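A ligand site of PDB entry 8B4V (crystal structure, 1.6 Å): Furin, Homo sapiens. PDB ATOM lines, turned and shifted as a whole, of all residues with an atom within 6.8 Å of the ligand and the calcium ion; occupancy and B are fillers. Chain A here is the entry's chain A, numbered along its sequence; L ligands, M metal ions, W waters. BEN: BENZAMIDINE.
A nitrogen (N1) of the ligand is in salt-bridge range of the side-chain carboxylate (OD2) of Asp 151, 3.8 Å away. OD2 of Asp 199 lies within salt-bridge range of N2 of the ligand (2.8 Å). N2 of the ligand sits at hydrogen-bond distance from O of Ala 185 (3.0 Å). The backbone carbonyl oxygen of Pro 149 lies within hydrogen-bond range of a nitrogen (N1) of the ligand, at 3.3 Å. The backbone carbonyl oxygen (O) of Trp 147 lies within hydrogen-bond range of a nitrogen (N2) of the ligand (3.4 Å).
The side-chain carboxylate of Asp 194 lies within salt-bridge range of the guanidinium group of Arg 412 (2.9 Å). The side-chain carboxylate of Asp 151 is in hydrogen-bond range of the backbone NH of Asn 188, at 2.9 Å. The backbone NH (N) of Asn 188 lies close to the side-chain carboxylate (OE1) of Glu 224, at 3.3 Å. The backbone NH (N) of Thr 202 is in hydrogen-bond range of the side-chain carboxylate (OD1) of Asp 199 (3.2 Å). The side-chain carboxylate (OD1) of Asp 199 lies within hydrogen-bond range of the backbone NH (N) of Tyr 201, 2.9 Å away. The side-chain amide oxygen of Asn 188 lies within hydrogen-bond range of the backbone NH of Thr 260 (2.8 Å). O of Trp 147 is in hydrogen-bond range of NE1 of Trp 184 (2.9 Å). The side-chain hydroxyl (OG1) of Thr 260 lies close to the backbone carbonyl oxygen (O) of Gly 187.
Water W2 lies within hydrogen-bond range of O of Ser 186, OD2 of Asp 199 and N1 of the ligand. Water W3 lies within hydrogen-bond range of OD1 of Asp 194 (3.1 Å) and O of Ser 195 (3.2 Å).
The calcium ion is bound by OD2 of Asp 194 (2.3 Å), OD1 of Asp 151 (2.4 Å), water W2 (2.4 Å), water W1 (2.4 Å), OE2 of Glu 224 (2.4 Å), water W3 (2.4 Å) and OE1 of Glu 224 (2.5 Å). The calcium ion has seven donor atoms within binding distance.
Merely in contact with the ligand: Asn 188, Ser 261, Gly 148, Gly 187, Ser 146, Thr 260 and Ser 186.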
ATOM      1  N   ALA A 145     -14.245 -12.690 -21.169  1.00  0.00           N
ATOM      2  CA  ALA A 145     -15.234 -11.625 -21.097  1.00  0.00           C
ATOM      3  C   ALA A 145     -14.624 -10.329 -21.599  1.00  0.00           C
ATOM      4  O   ALA A 145     -13.652  -9.832 -21.023  1.00  0.00           O
ATOM      5  CB  ALA A 145     -15.773 -11.457 -19.671  1.00  0.00           C
ATOM      6  N   SER A 146     -15.189  -9.831 -22.700  1.00  0.00           N
ATOM      7  CA  SER A 146     -14.783  -8.628 -23.419  1.00  0.00           C
ATOM      8  C   SER A 146     -15.882  -7.578 -23.221  1.00  0.00           C
ATOM      9  O   SER A 146     -16.448  -7.098 -24.207  1.00  0.00           O
ATOM     10  CB  SER A 146     -14.577  -8.921 -24.909  1.00  0.00           C
ATOM     11  OG  SER A 146     -13.531  -9.845 -25.144  1.00  0.00           O
ATOM     12  N   TRP A 147     -16.213  -7.264 -21.969  1.00  0.00           N
ATOM     13  CA  TRP A 147     -17.299  -6.364 -21.607  1.00  0.00           C
ATOM     14  C   TRP A 147     -17.036  -5.877 -20.189  1.00  0.00           C
ATOM     15  O   TRP A 147     -16.138  -6.366 -19.503  1.00  0.00           O
ATOM     16  CB  TRP A 147     -18.695  -7.034 -21.687  1.00  0.00           C
ATOM     17  CG  TRP A 147     -18.898  -8.389 -20.971  1.00  0.00           C
ATOM     18  CD1 TRP A 147     -18.792  -9.617 -21.535  1.00  0.00           C
ATOM     19  CD2 TRP A 147     -19.273  -8.617 -19.589  1.00  0.00           C
ATOM     20  NE1 TRP A 147     -19.042 -10.600 -20.617  1.00  0.00           N
ATOM     21  CE2 TRP A 147     -19.341 -10.024 -19.415  1.00  0.00           C
ATOM     22  CE3 TRP A 147     -19.535  -7.787 -18.502  1.00  0.00           C
ATOM     23  CZ2 TRP A 147     -19.668 -10.601 -18.196  1.00  0.00           C
ATOM     24  CZ3 TRP A 147     -19.860  -8.379 -17.282  1.00  0.00           C
ATOM     25  CH2 TRP A 147     -19.911  -9.769 -17.146  1.00  0.00           C
ATOM     26  N   GLY A 148     -17.833  -4.881 -19.748  1.00  0.00           N
ATOM     27  CA  GLY A 148     -17.786  -4.362 -18.387  1.00  0.00           C
ATOM     28  C   GLY A 148     -18.482  -3.013 -18.221  1.00  0.00           C
ATOM     29  O   GLY A 148     -19.222  -2.575 -19.113  1.00  0.00           O
ATOM     30  N   PRO A 149     -18.238  -2.309 -17.107  1.00  0.00           N
ATOM     31  CA  PRO A 149     -18.892  -1.002 -16.897  1.00  0.00           C
ATOM     32  C   PRO A 149     -18.558  -0.003 -18.006  1.00  0.00           C
ATOM     33  O   PRO A 149     -17.501  -0.083 -18.624  1.00  0.00           O
ATOM     34  CB  PRO A 149     -18.340  -0.510 -15.559  1.00  0.00           C
ATOM     35  CG  PRO A 149     -17.522  -1.613 -15.009  1.00  0.00           C
ATOM     36  CD  PRO A 149     -17.307  -2.665 -16.024  1.00  0.00           C
ATOM     37  N   GLU A 150     -19.468   0.945 -18.216  1.00  0.00           N
ATOM     38  CA  GLU A 150     -19.332   1.895 -19.319  1.00  0.00           C
ATOM     39  C   GLU A 150     -17.960   2.565 -19.294  1.00  0.00           C
ATOM     40  O   GLU A 150     -17.514   3.072 -18.262  1.00  0.00           O
ATOM     41  CB  GLU A 150     -20.426   2.956 -19.248  1.00  0.00           C
ATOM     42  CG  GLU A 150     -20.397   3.921 -20.427  1.00  0.00           C
ATOM     43  CD  GLU A 150     -21.670   4.735 -20.578  1.00  0.00           C
ATOM     44  OE1 GLU A 150     -22.546   4.655 -19.684  1.00  0.00           O
ATOM     45  OE2 GLU A 150     -21.791   5.450 -21.591  1.00  0.00           O
ATOM     46  N   ASP A 151     -17.291   2.544 -20.445  1.00  0.00           N
ATOM     47  CA  ASP A 151     -15.957   3.130 -20.600  1.00  0.00           C
ATOM     48  C   ASP A 151     -16.026   4.616 -20.920  1.00  0.00           C
ATOM     49  O   ASP A 151     -15.367   5.110 -21.839  1.00  0.00           O
ATOM     50  CB  ASP A 151     -15.191   2.388 -21.699  1.00  0.00           C
ATOM     51  CG  ASP A 151     -14.730   0.995 -21.287  1.00  0.00           C
ATOM     52  OD1 ASP A 151     -14.514   0.763 -20.079  1.00  0.00           O
ATOM     53  OD2 ASP A 151     -14.534   0.145 -22.199  1.00  0.00           O
ATOM     54  N   ASP A 152     -16.836   5.362 -20.153  1.00  0.00           N
ATOM     55  CA  ASP A 152     -17.008   6.789 -20.397  1.00  0.00           C
ATOM     56  C   ASP A 152     -16.009   7.641 -19.629  1.00  0.00           C
ATOM     57  O   ASP A 152     -16.014   8.863 -19.799  1.00  0.00           O
ATOM     58  CB  ASP A 152     -18.444   7.245 -20.079  1.00  0.00           C
ATOM     59  CG  ASP A 152     -18.896   6.904 -18.668  1.00  0.00           C
ATOM     60  OD1 ASP A 152     -18.075   6.471 -17.829  1.00  0.00           O
ATOM     61  OD2 ASP A 152     -20.099   7.091 -18.392  1.00  0.00           O
ATOM     62  N   GLY A 153     -15.143   7.021 -18.819  1.00  0.00           N
ATOM     63  CA  GLY A 153     -14.189   7.780 -18.051  1.00  0.00           C
ATOM     64  C   GLY A 153     -14.779   8.498 -16.874  1.00  0.00           C
ATOM     65  O   GLY A 153     -14.127   9.364 -16.292  1.00  0.00           O
ATOM     66  N   THR A 155     -17.276   6.496 -14.743  1.00  0.00           N
ATOM     67  CA  THR A 155     -17.983   5.471 -13.986  1.00  0.00           C
ATOM     68  C   THR A 155     -17.026   4.749 -13.048  1.00  0.00           C
ATOM     69  O   THR A 155     -15.872   4.471 -13.417  1.00  0.00           O
ATOM     70  CB  THR A 155     -18.636   4.499 -14.966  1.00  0.00           C
ATOM     71  OG1 THR A 155     -19.551   5.217 -15.812  1.00  0.00           O
ATOM     72  CG2 THR A 155     -19.393   3.400 -14.242  1.00  0.00           C
ATOM     73  N   TRP A 184     -10.154 -11.431 -18.706  1.00  0.00           N
ATOM     74  CA  TRP A 184     -10.910 -10.188 -18.858  1.00  0.00           C
ATOM     75  C   TRP A 184     -10.162  -9.181 -19.718  1.00  0.00           C
ATOM     76  O   TRP A 184      -8.952  -9.031 -19.596  1.00  0.00           O
ATOM     77  CB  TRP A 184     -11.210  -9.513 -17.477  1.00  0.00           C
ATOM     78  CG  TRP A 184     -12.627  -9.040 -17.416  1.00  0.00           C
ATOM     79  CD1 TRP A 184     -13.109  -7.822 -17.797  1.00  0.00           C
ATOM     80  CD2 TRP A 184     -13.756  -9.805 -16.990  1.00  0.00           C
ATOM     81  NE1 TRP A 184     -14.486  -7.784 -17.638  1.00  0.00           N
ATOM     82  CE2 TRP A 184     -14.891  -8.994 -17.127  1.00  0.00           C
ATOM     83  CE3 TRP A 184     -13.904 -11.107 -16.490  1.00  0.00           C
ATOM     84  CZ2 TRP A 184     -16.167  -9.435 -16.791  1.00  0.00           C
ATOM     85  CZ3 TRP A 184     -15.172 -11.539 -16.147  1.00  0.00           C
ATOM     86  CH2 TRP A 184     -16.285 -10.711 -16.302  1.00  0.00           C
ATOM     87  N   ALA A 185     -10.911  -8.478 -20.567  1.00  0.00           N
ATOM     88  CA  ALA A 185     -10.384  -7.340 -21.315  1.00  0.00           C
ATOM     89  C   ALA A 185     -10.352  -6.113 -20.403  1.00  0.00           C
ATOM     90  O   ALA A 185     -11.346  -5.805 -19.747  1.00  0.00           O
ATOM     91  CB  ALA A 185     -11.256  -7.036 -22.534  1.00  0.00           C
ATOM     92  N   SER A 186      -9.232  -5.386 -20.396  1.00  0.00           N
ATOM     93  CA  SER A 186      -9.094  -4.331 -19.395  1.00  0.00           C
ATOM     94  C   SER A 186      -9.889  -3.065 -19.695  1.00  0.00           C
ATOM     95  O   SER A 186     -10.019  -2.225 -18.790  1.00  0.00           O
ATOM     96  CB  SER A 186      -7.621  -3.953 -19.188  1.00  0.00           C
ATOM     97  OG  SER A 186      -7.028  -3.465 -20.390  1.00  0.00           O
ATOM     98  N   GLY A 187     -10.389  -2.875 -20.904  1.00  0.00           N
ATOM     99  CA  GLY A 187     -11.218  -1.723 -21.205  1.00  0.00           C
ATOM    100  C   GLY A 187     -10.867  -1.036 -22.512  1.00  0.00           C
ATOM    101  O   GLY A 187      -9.750  -1.117 -23.022  1.00  0.00           O
ATOM    102  N   ASN A 188     -11.855  -0.329 -23.077  1.00  0.00           N
ATOM    103  CA  ASN A 188     -11.689   0.384 -24.335  1.00  0.00           C
ATOM    104  C   ASN A 188     -11.895   1.890 -24.192  1.00  0.00           C
ATOM    105  O   ASN A 188     -12.211   2.571 -25.179  1.00  0.00           O
ATOM    106  CB  ASN A 188     -12.646  -0.155 -25.401  1.00  0.00           C
ATOM    107  CG  ASN A 188     -12.268  -1.534 -25.883  1.00  0.00           C
ATOM    108  OD1 ASN A 188     -11.095  -1.871 -25.962  1.00  0.00           O
ATOM    109  ND2 ASN A 188     -13.267  -2.344 -26.218  1.00  0.00           N
ATOM    110  N   GLY A 189     -11.676   2.434 -22.996  1.00  0.00           N
ATOM    111  CA  GLY A 189     -11.987   3.825 -22.710  1.00  0.00           C
ATOM    112  C   GLY A 189     -10.869   4.840 -22.882  1.00  0.00           C
ATOM    113  O   GLY A 189     -10.953   5.949 -22.334  1.00  0.00           O
ATOM    114  N   ASP A 194     -10.065   6.998 -19.595  1.00  0.00           N
ATOM    115  CA  ASP A 194     -10.512   6.114 -18.526  1.00  0.00           C
ATOM    116  C   ASP A 194      -9.313   5.411 -17.874  1.00  0.00           C
ATOM    117  O   ASP A 194      -8.261   5.237 -18.484  1.00  0.00           O
ATOM    118  CB  ASP A 194     -11.519   5.102 -19.082  1.00  0.00           C
ATOM    119  CG  ASP A 194     -12.442   4.502 -18.029  1.00  0.00           C
ATOM    120  OD1 ASP A 194     -12.352   4.872 -16.835  1.00  0.00           O
ATOM    121  OD2 ASP A 194     -13.256   3.630 -18.400  1.00  0.00           O
ATOM    122  N   SER A 195      -9.509   5.001 -16.621  1.00  0.00           N
ATOM    123  CA  SER A 195      -8.466   4.450 -15.752  1.00  0.00           C
ATOM    124  C   SER A 195      -9.068   3.141 -15.230  1.00  0.00           C
ATOM    125  O   SER A 195     -10.086   3.166 -14.535  1.00  0.00           O
ATOM    126  CB  SER A 195      -8.137   5.441 -14.643  1.00  0.00           C
ATOM    127  OG  SER A 195      -6.941   5.156 -13.919  1.00  0.00           O
ATOM    128  N   CYS A 196      -8.472   1.991 -15.603  1.00  0.00           N
ATOM    129  CA  CYS A 196      -9.235   0.747 -15.521  1.00  0.00           C
ATOM    130  C   CYS A 196      -9.320   0.154 -14.118  1.00  0.00           C
ATOM    131  O   CYS A 196     -10.030  -0.841 -13.946  1.00  0.00           O
ATOM    132  CB  CYS A 196      -8.691  -0.310 -16.512  1.00  0.00           C
ATOM    133  SG  CYS A 196      -6.912  -0.456 -16.835  1.00  0.00           S
ATOM    134  N   CYS A 198     -11.018   1.585 -12.037  1.00  0.00           N
ATOM    135  CA  CYS A 198     -12.388   1.987 -11.754  1.00  0.00           C
ATOM    136  C   CYS A 198     -13.430   1.005 -12.282  1.00  0.00           C
ATOM    137  O   CYS A 198     -14.634   1.267 -12.147  1.00  0.00           O
ATOM    138  CB  CYS A 198     -12.664   3.385 -12.321  1.00  0.00           C
ATOM    139  SG  CYS A 198     -11.729   4.709 -11.531  1.00  0.00           S
ATOM    140  N   ASP A 199     -12.980  -0.113 -12.857  1.00  0.00           N
ATOM    141  CA  ASP A 199     -13.786  -1.204 -13.379  1.00  0.00           C
ATOM    142  C   ASP A 199     -13.519  -2.391 -12.462  1.00  0.00           C
ATOM    143  O   ASP A 199     -12.424  -2.955 -12.479  1.00  0.00           O
ATOM    144  CB  ASP A 199     -13.381  -1.425 -14.836  1.00  0.00           C
ATOM    145  CG  ASP A 199     -13.915  -2.701 -15.449  1.00  0.00           C
ATOM    146  OD1 ASP A 199     -14.358  -3.617 -14.722  1.00  0.00           O
ATOM    147  OD2 ASP A 199     -13.858  -2.790 -16.696  1.00  0.00           O
ATOM    148  N   TYR A 201     -14.547  -5.377 -12.436  1.00  0.00           N
ATOM    149  CA  TYR A 201     -14.362  -6.693 -13.036  1.00  0.00           C
ATOM    150  C   TYR A 201     -12.895  -6.909 -13.393  1.00  0.00           C
ATOM    151  O   TYR A 201     -12.293  -7.904 -12.990  1.00  0.00           O
ATOM    152  CB  TYR A 201     -15.259  -6.840 -14.286  1.00  0.00           C
ATOM    153  CG  TYR A 201     -16.727  -6.683 -13.966  1.00  0.00           C
ATOM    154  CD1 TYR A 201     -17.309  -5.432 -13.875  1.00  0.00           C
ATOM    155  CD2 TYR A 201     -17.536  -7.793 -13.736  1.00  0.00           C
ATOM    156  CE1 TYR A 201     -18.642  -5.273 -13.572  1.00  0.00           C
ATOM    157  CE2 TYR A 201     -18.892  -7.653 -13.425  1.00  0.00           C
ATOM    158  CZ  TYR A 201     -19.429  -6.387 -13.348  1.00  0.00           C
ATOM    159  OH  TYR A 201     -20.766  -6.180 -13.058  1.00  0.00           O
ATOM    160  N   THR A 202     -12.285  -5.949 -14.086  1.00  0.00           N
ATOM    161  CA  THR A 202     -10.869  -6.108 -14.412  1.00  0.00           C
ATOM    162  C   THR A 202      -9.985  -5.885 -13.187  1.00  0.00           C
ATOM    163  O   THR A 202      -8.941  -6.540 -13.068  1.00  0.00           O
ATOM    164  CB  THR A 202     -10.507  -5.178 -15.566  1.00  0.00           C
ATOM    165  OG1 THR A 202      -9.226  -5.561 -16.097  1.00  0.00           O
ATOM    166  CG2 THR A 202     -10.547  -3.735 -15.140  1.00  0.00           C
ATOM    167  N   GLU A 224      -6.685   1.620 -21.769  1.00  0.00           N
ATOM    168  CA  GLU A 224      -6.726   2.160 -20.417  1.00  0.00           C
ATOM    169  C   GLU A 224      -5.521   1.633 -19.646  1.00  0.00           C
ATOM    170  O   GLU A 224      -5.273   0.428 -19.628  1.00  0.00           O
ATOM    171  CB  GLU A 224      -8.002   1.759 -19.700  1.00  0.00           C
ATOM    172  CG  GLU A 224      -9.277   2.233 -20.385  1.00  0.00           C
ATOM    173  CD  GLU A 224     -10.557   1.826 -19.655  1.00  0.00           C
ATOM    174  OE1 GLU A 224     -11.544   1.480 -20.354  1.00  0.00           O
ATOM    175  OE2 GLU A 224     -10.614   1.878 -18.406  1.00  0.00           O
ATOM    176  N   GLY A 259      -9.760  -3.658 -30.660  1.00  0.00           N
ATOM    177  CA  GLY A 259      -9.899  -3.264 -29.269  1.00  0.00           C
ATOM    178  C   GLY A 259      -9.365  -4.280 -28.284  1.00  0.00           C
ATOM    179  O   GLY A 259      -8.901  -5.360 -28.637  1.00  0.00           O
ATOM    180  N   THR A 260      -9.441  -3.928 -26.981  1.00  0.00           N
ATOM    181  CA  THR A 260      -9.034  -4.916 -25.983  1.00  0.00           C
ATOM    182  C   THR A 260     -10.009  -6.099 -25.982  1.00  0.00           C
ATOM    183  O   THR A 260      -9.661  -7.177 -25.471  1.00  0.00           O
ATOM    184  CB  THR A 260      -8.957  -4.360 -24.551  1.00  0.00           C
ATOM    185  OG1 THR A 260     -10.261  -4.090 -24.036  1.00  0.00           O
ATOM    186  CG2 THR A 260      -8.109  -3.112 -24.490  1.00  0.00           C
ATOM    187  N   SER A 261     -11.209  -5.917 -26.550  1.00  0.00           N
ATOM    188  CA  SER A 261     -12.145  -7.018 -26.702  1.00  0.00           C
ATOM    189  C   SER A 261     -11.556  -8.170 -27.511  1.00  0.00           C
ATOM    190  O   SER A 261     -11.964  -9.320 -27.336  1.00  0.00           O
ATOM    191  CB  SER A 261     -13.409  -6.522 -27.413  1.00  0.00           C
ATOM    192  OG  SER A 261     -13.876  -5.328 -26.829  1.00  0.00           O
ATOM    193  N   ARG A 412      -9.038  11.583 -14.182  1.00  0.00           N
ATOM    194  CA  ARG A 412     -10.063  11.293 -15.186  1.00  0.00           C
ATOM    195  C   ARG A 412     -10.815  12.581 -15.478  1.00  0.00           C
ATOM    196  O   ARG A 412     -11.692  12.992 -14.697  1.00  0.00           O
ATOM    197  CB  ARG A 412     -11.009  10.196 -14.701  1.00  0.00           C
ATOM    198  CG  ARG A 412     -10.344   8.827 -14.650  1.00  0.00           C
ATOM    199  CD  ARG A 412     -11.329   7.662 -14.700  1.00  0.00           C
ATOM    200  NE  ARG A 412     -12.355   7.747 -13.664  1.00  0.00           N
ATOM    201  CZ  ARG A 412     -13.456   7.003 -13.643  1.00  0.00           C
ATOM    202  NH1 ARG A 412     -14.360   7.172 -12.679  1.00  0.00           N
ATOM    203  NH2 ARG A 412     -13.656   6.104 -14.587  1.00  0.00           N
HETATM  204  C1  BEN L   1     -14.650  -3.414 -21.255  1.00  0.00           C
HETATM  205  C2  BEN L   1     -15.767  -2.890 -21.904  1.00  0.00           C
HETATM  206  C3  BEN L   1     -15.958  -3.090 -23.271  1.00  0.00           C
HETATM  207  C4  BEN L   1     -15.022  -3.812 -24.002  1.00  0.00           C
HETATM  208  C5  BEN L   1     -13.903  -4.344 -23.374  1.00  0.00           C
HETATM  209  C6  BEN L   1     -13.720  -4.138 -22.005  1.00  0.00           C
HETATM  210  C   BEN L   1     -14.470  -3.215 -19.874  1.00  0.00           C
HETATM  211  N1  BEN L   1     -15.125  -2.211 -19.275  1.00  0.00           N
HETATM  212  N2  BEN L   1     -13.666  -4.051 -19.196  1.00  0.00           N
HETATM  213 CA    CA M   1     -12.973   1.318 -18.354  1.00  0.00          CA
HETATM  214  O   HOH W   1     -15.089   0.870 -17.265  1.00  0.00           O
HETATM  215  O   HOH W   2     -12.217  -0.899 -17.905  1.00  0.00           O
HETATM  216  O   HOH W   3     -12.656   1.895 -16.001  1.00  0.00           O
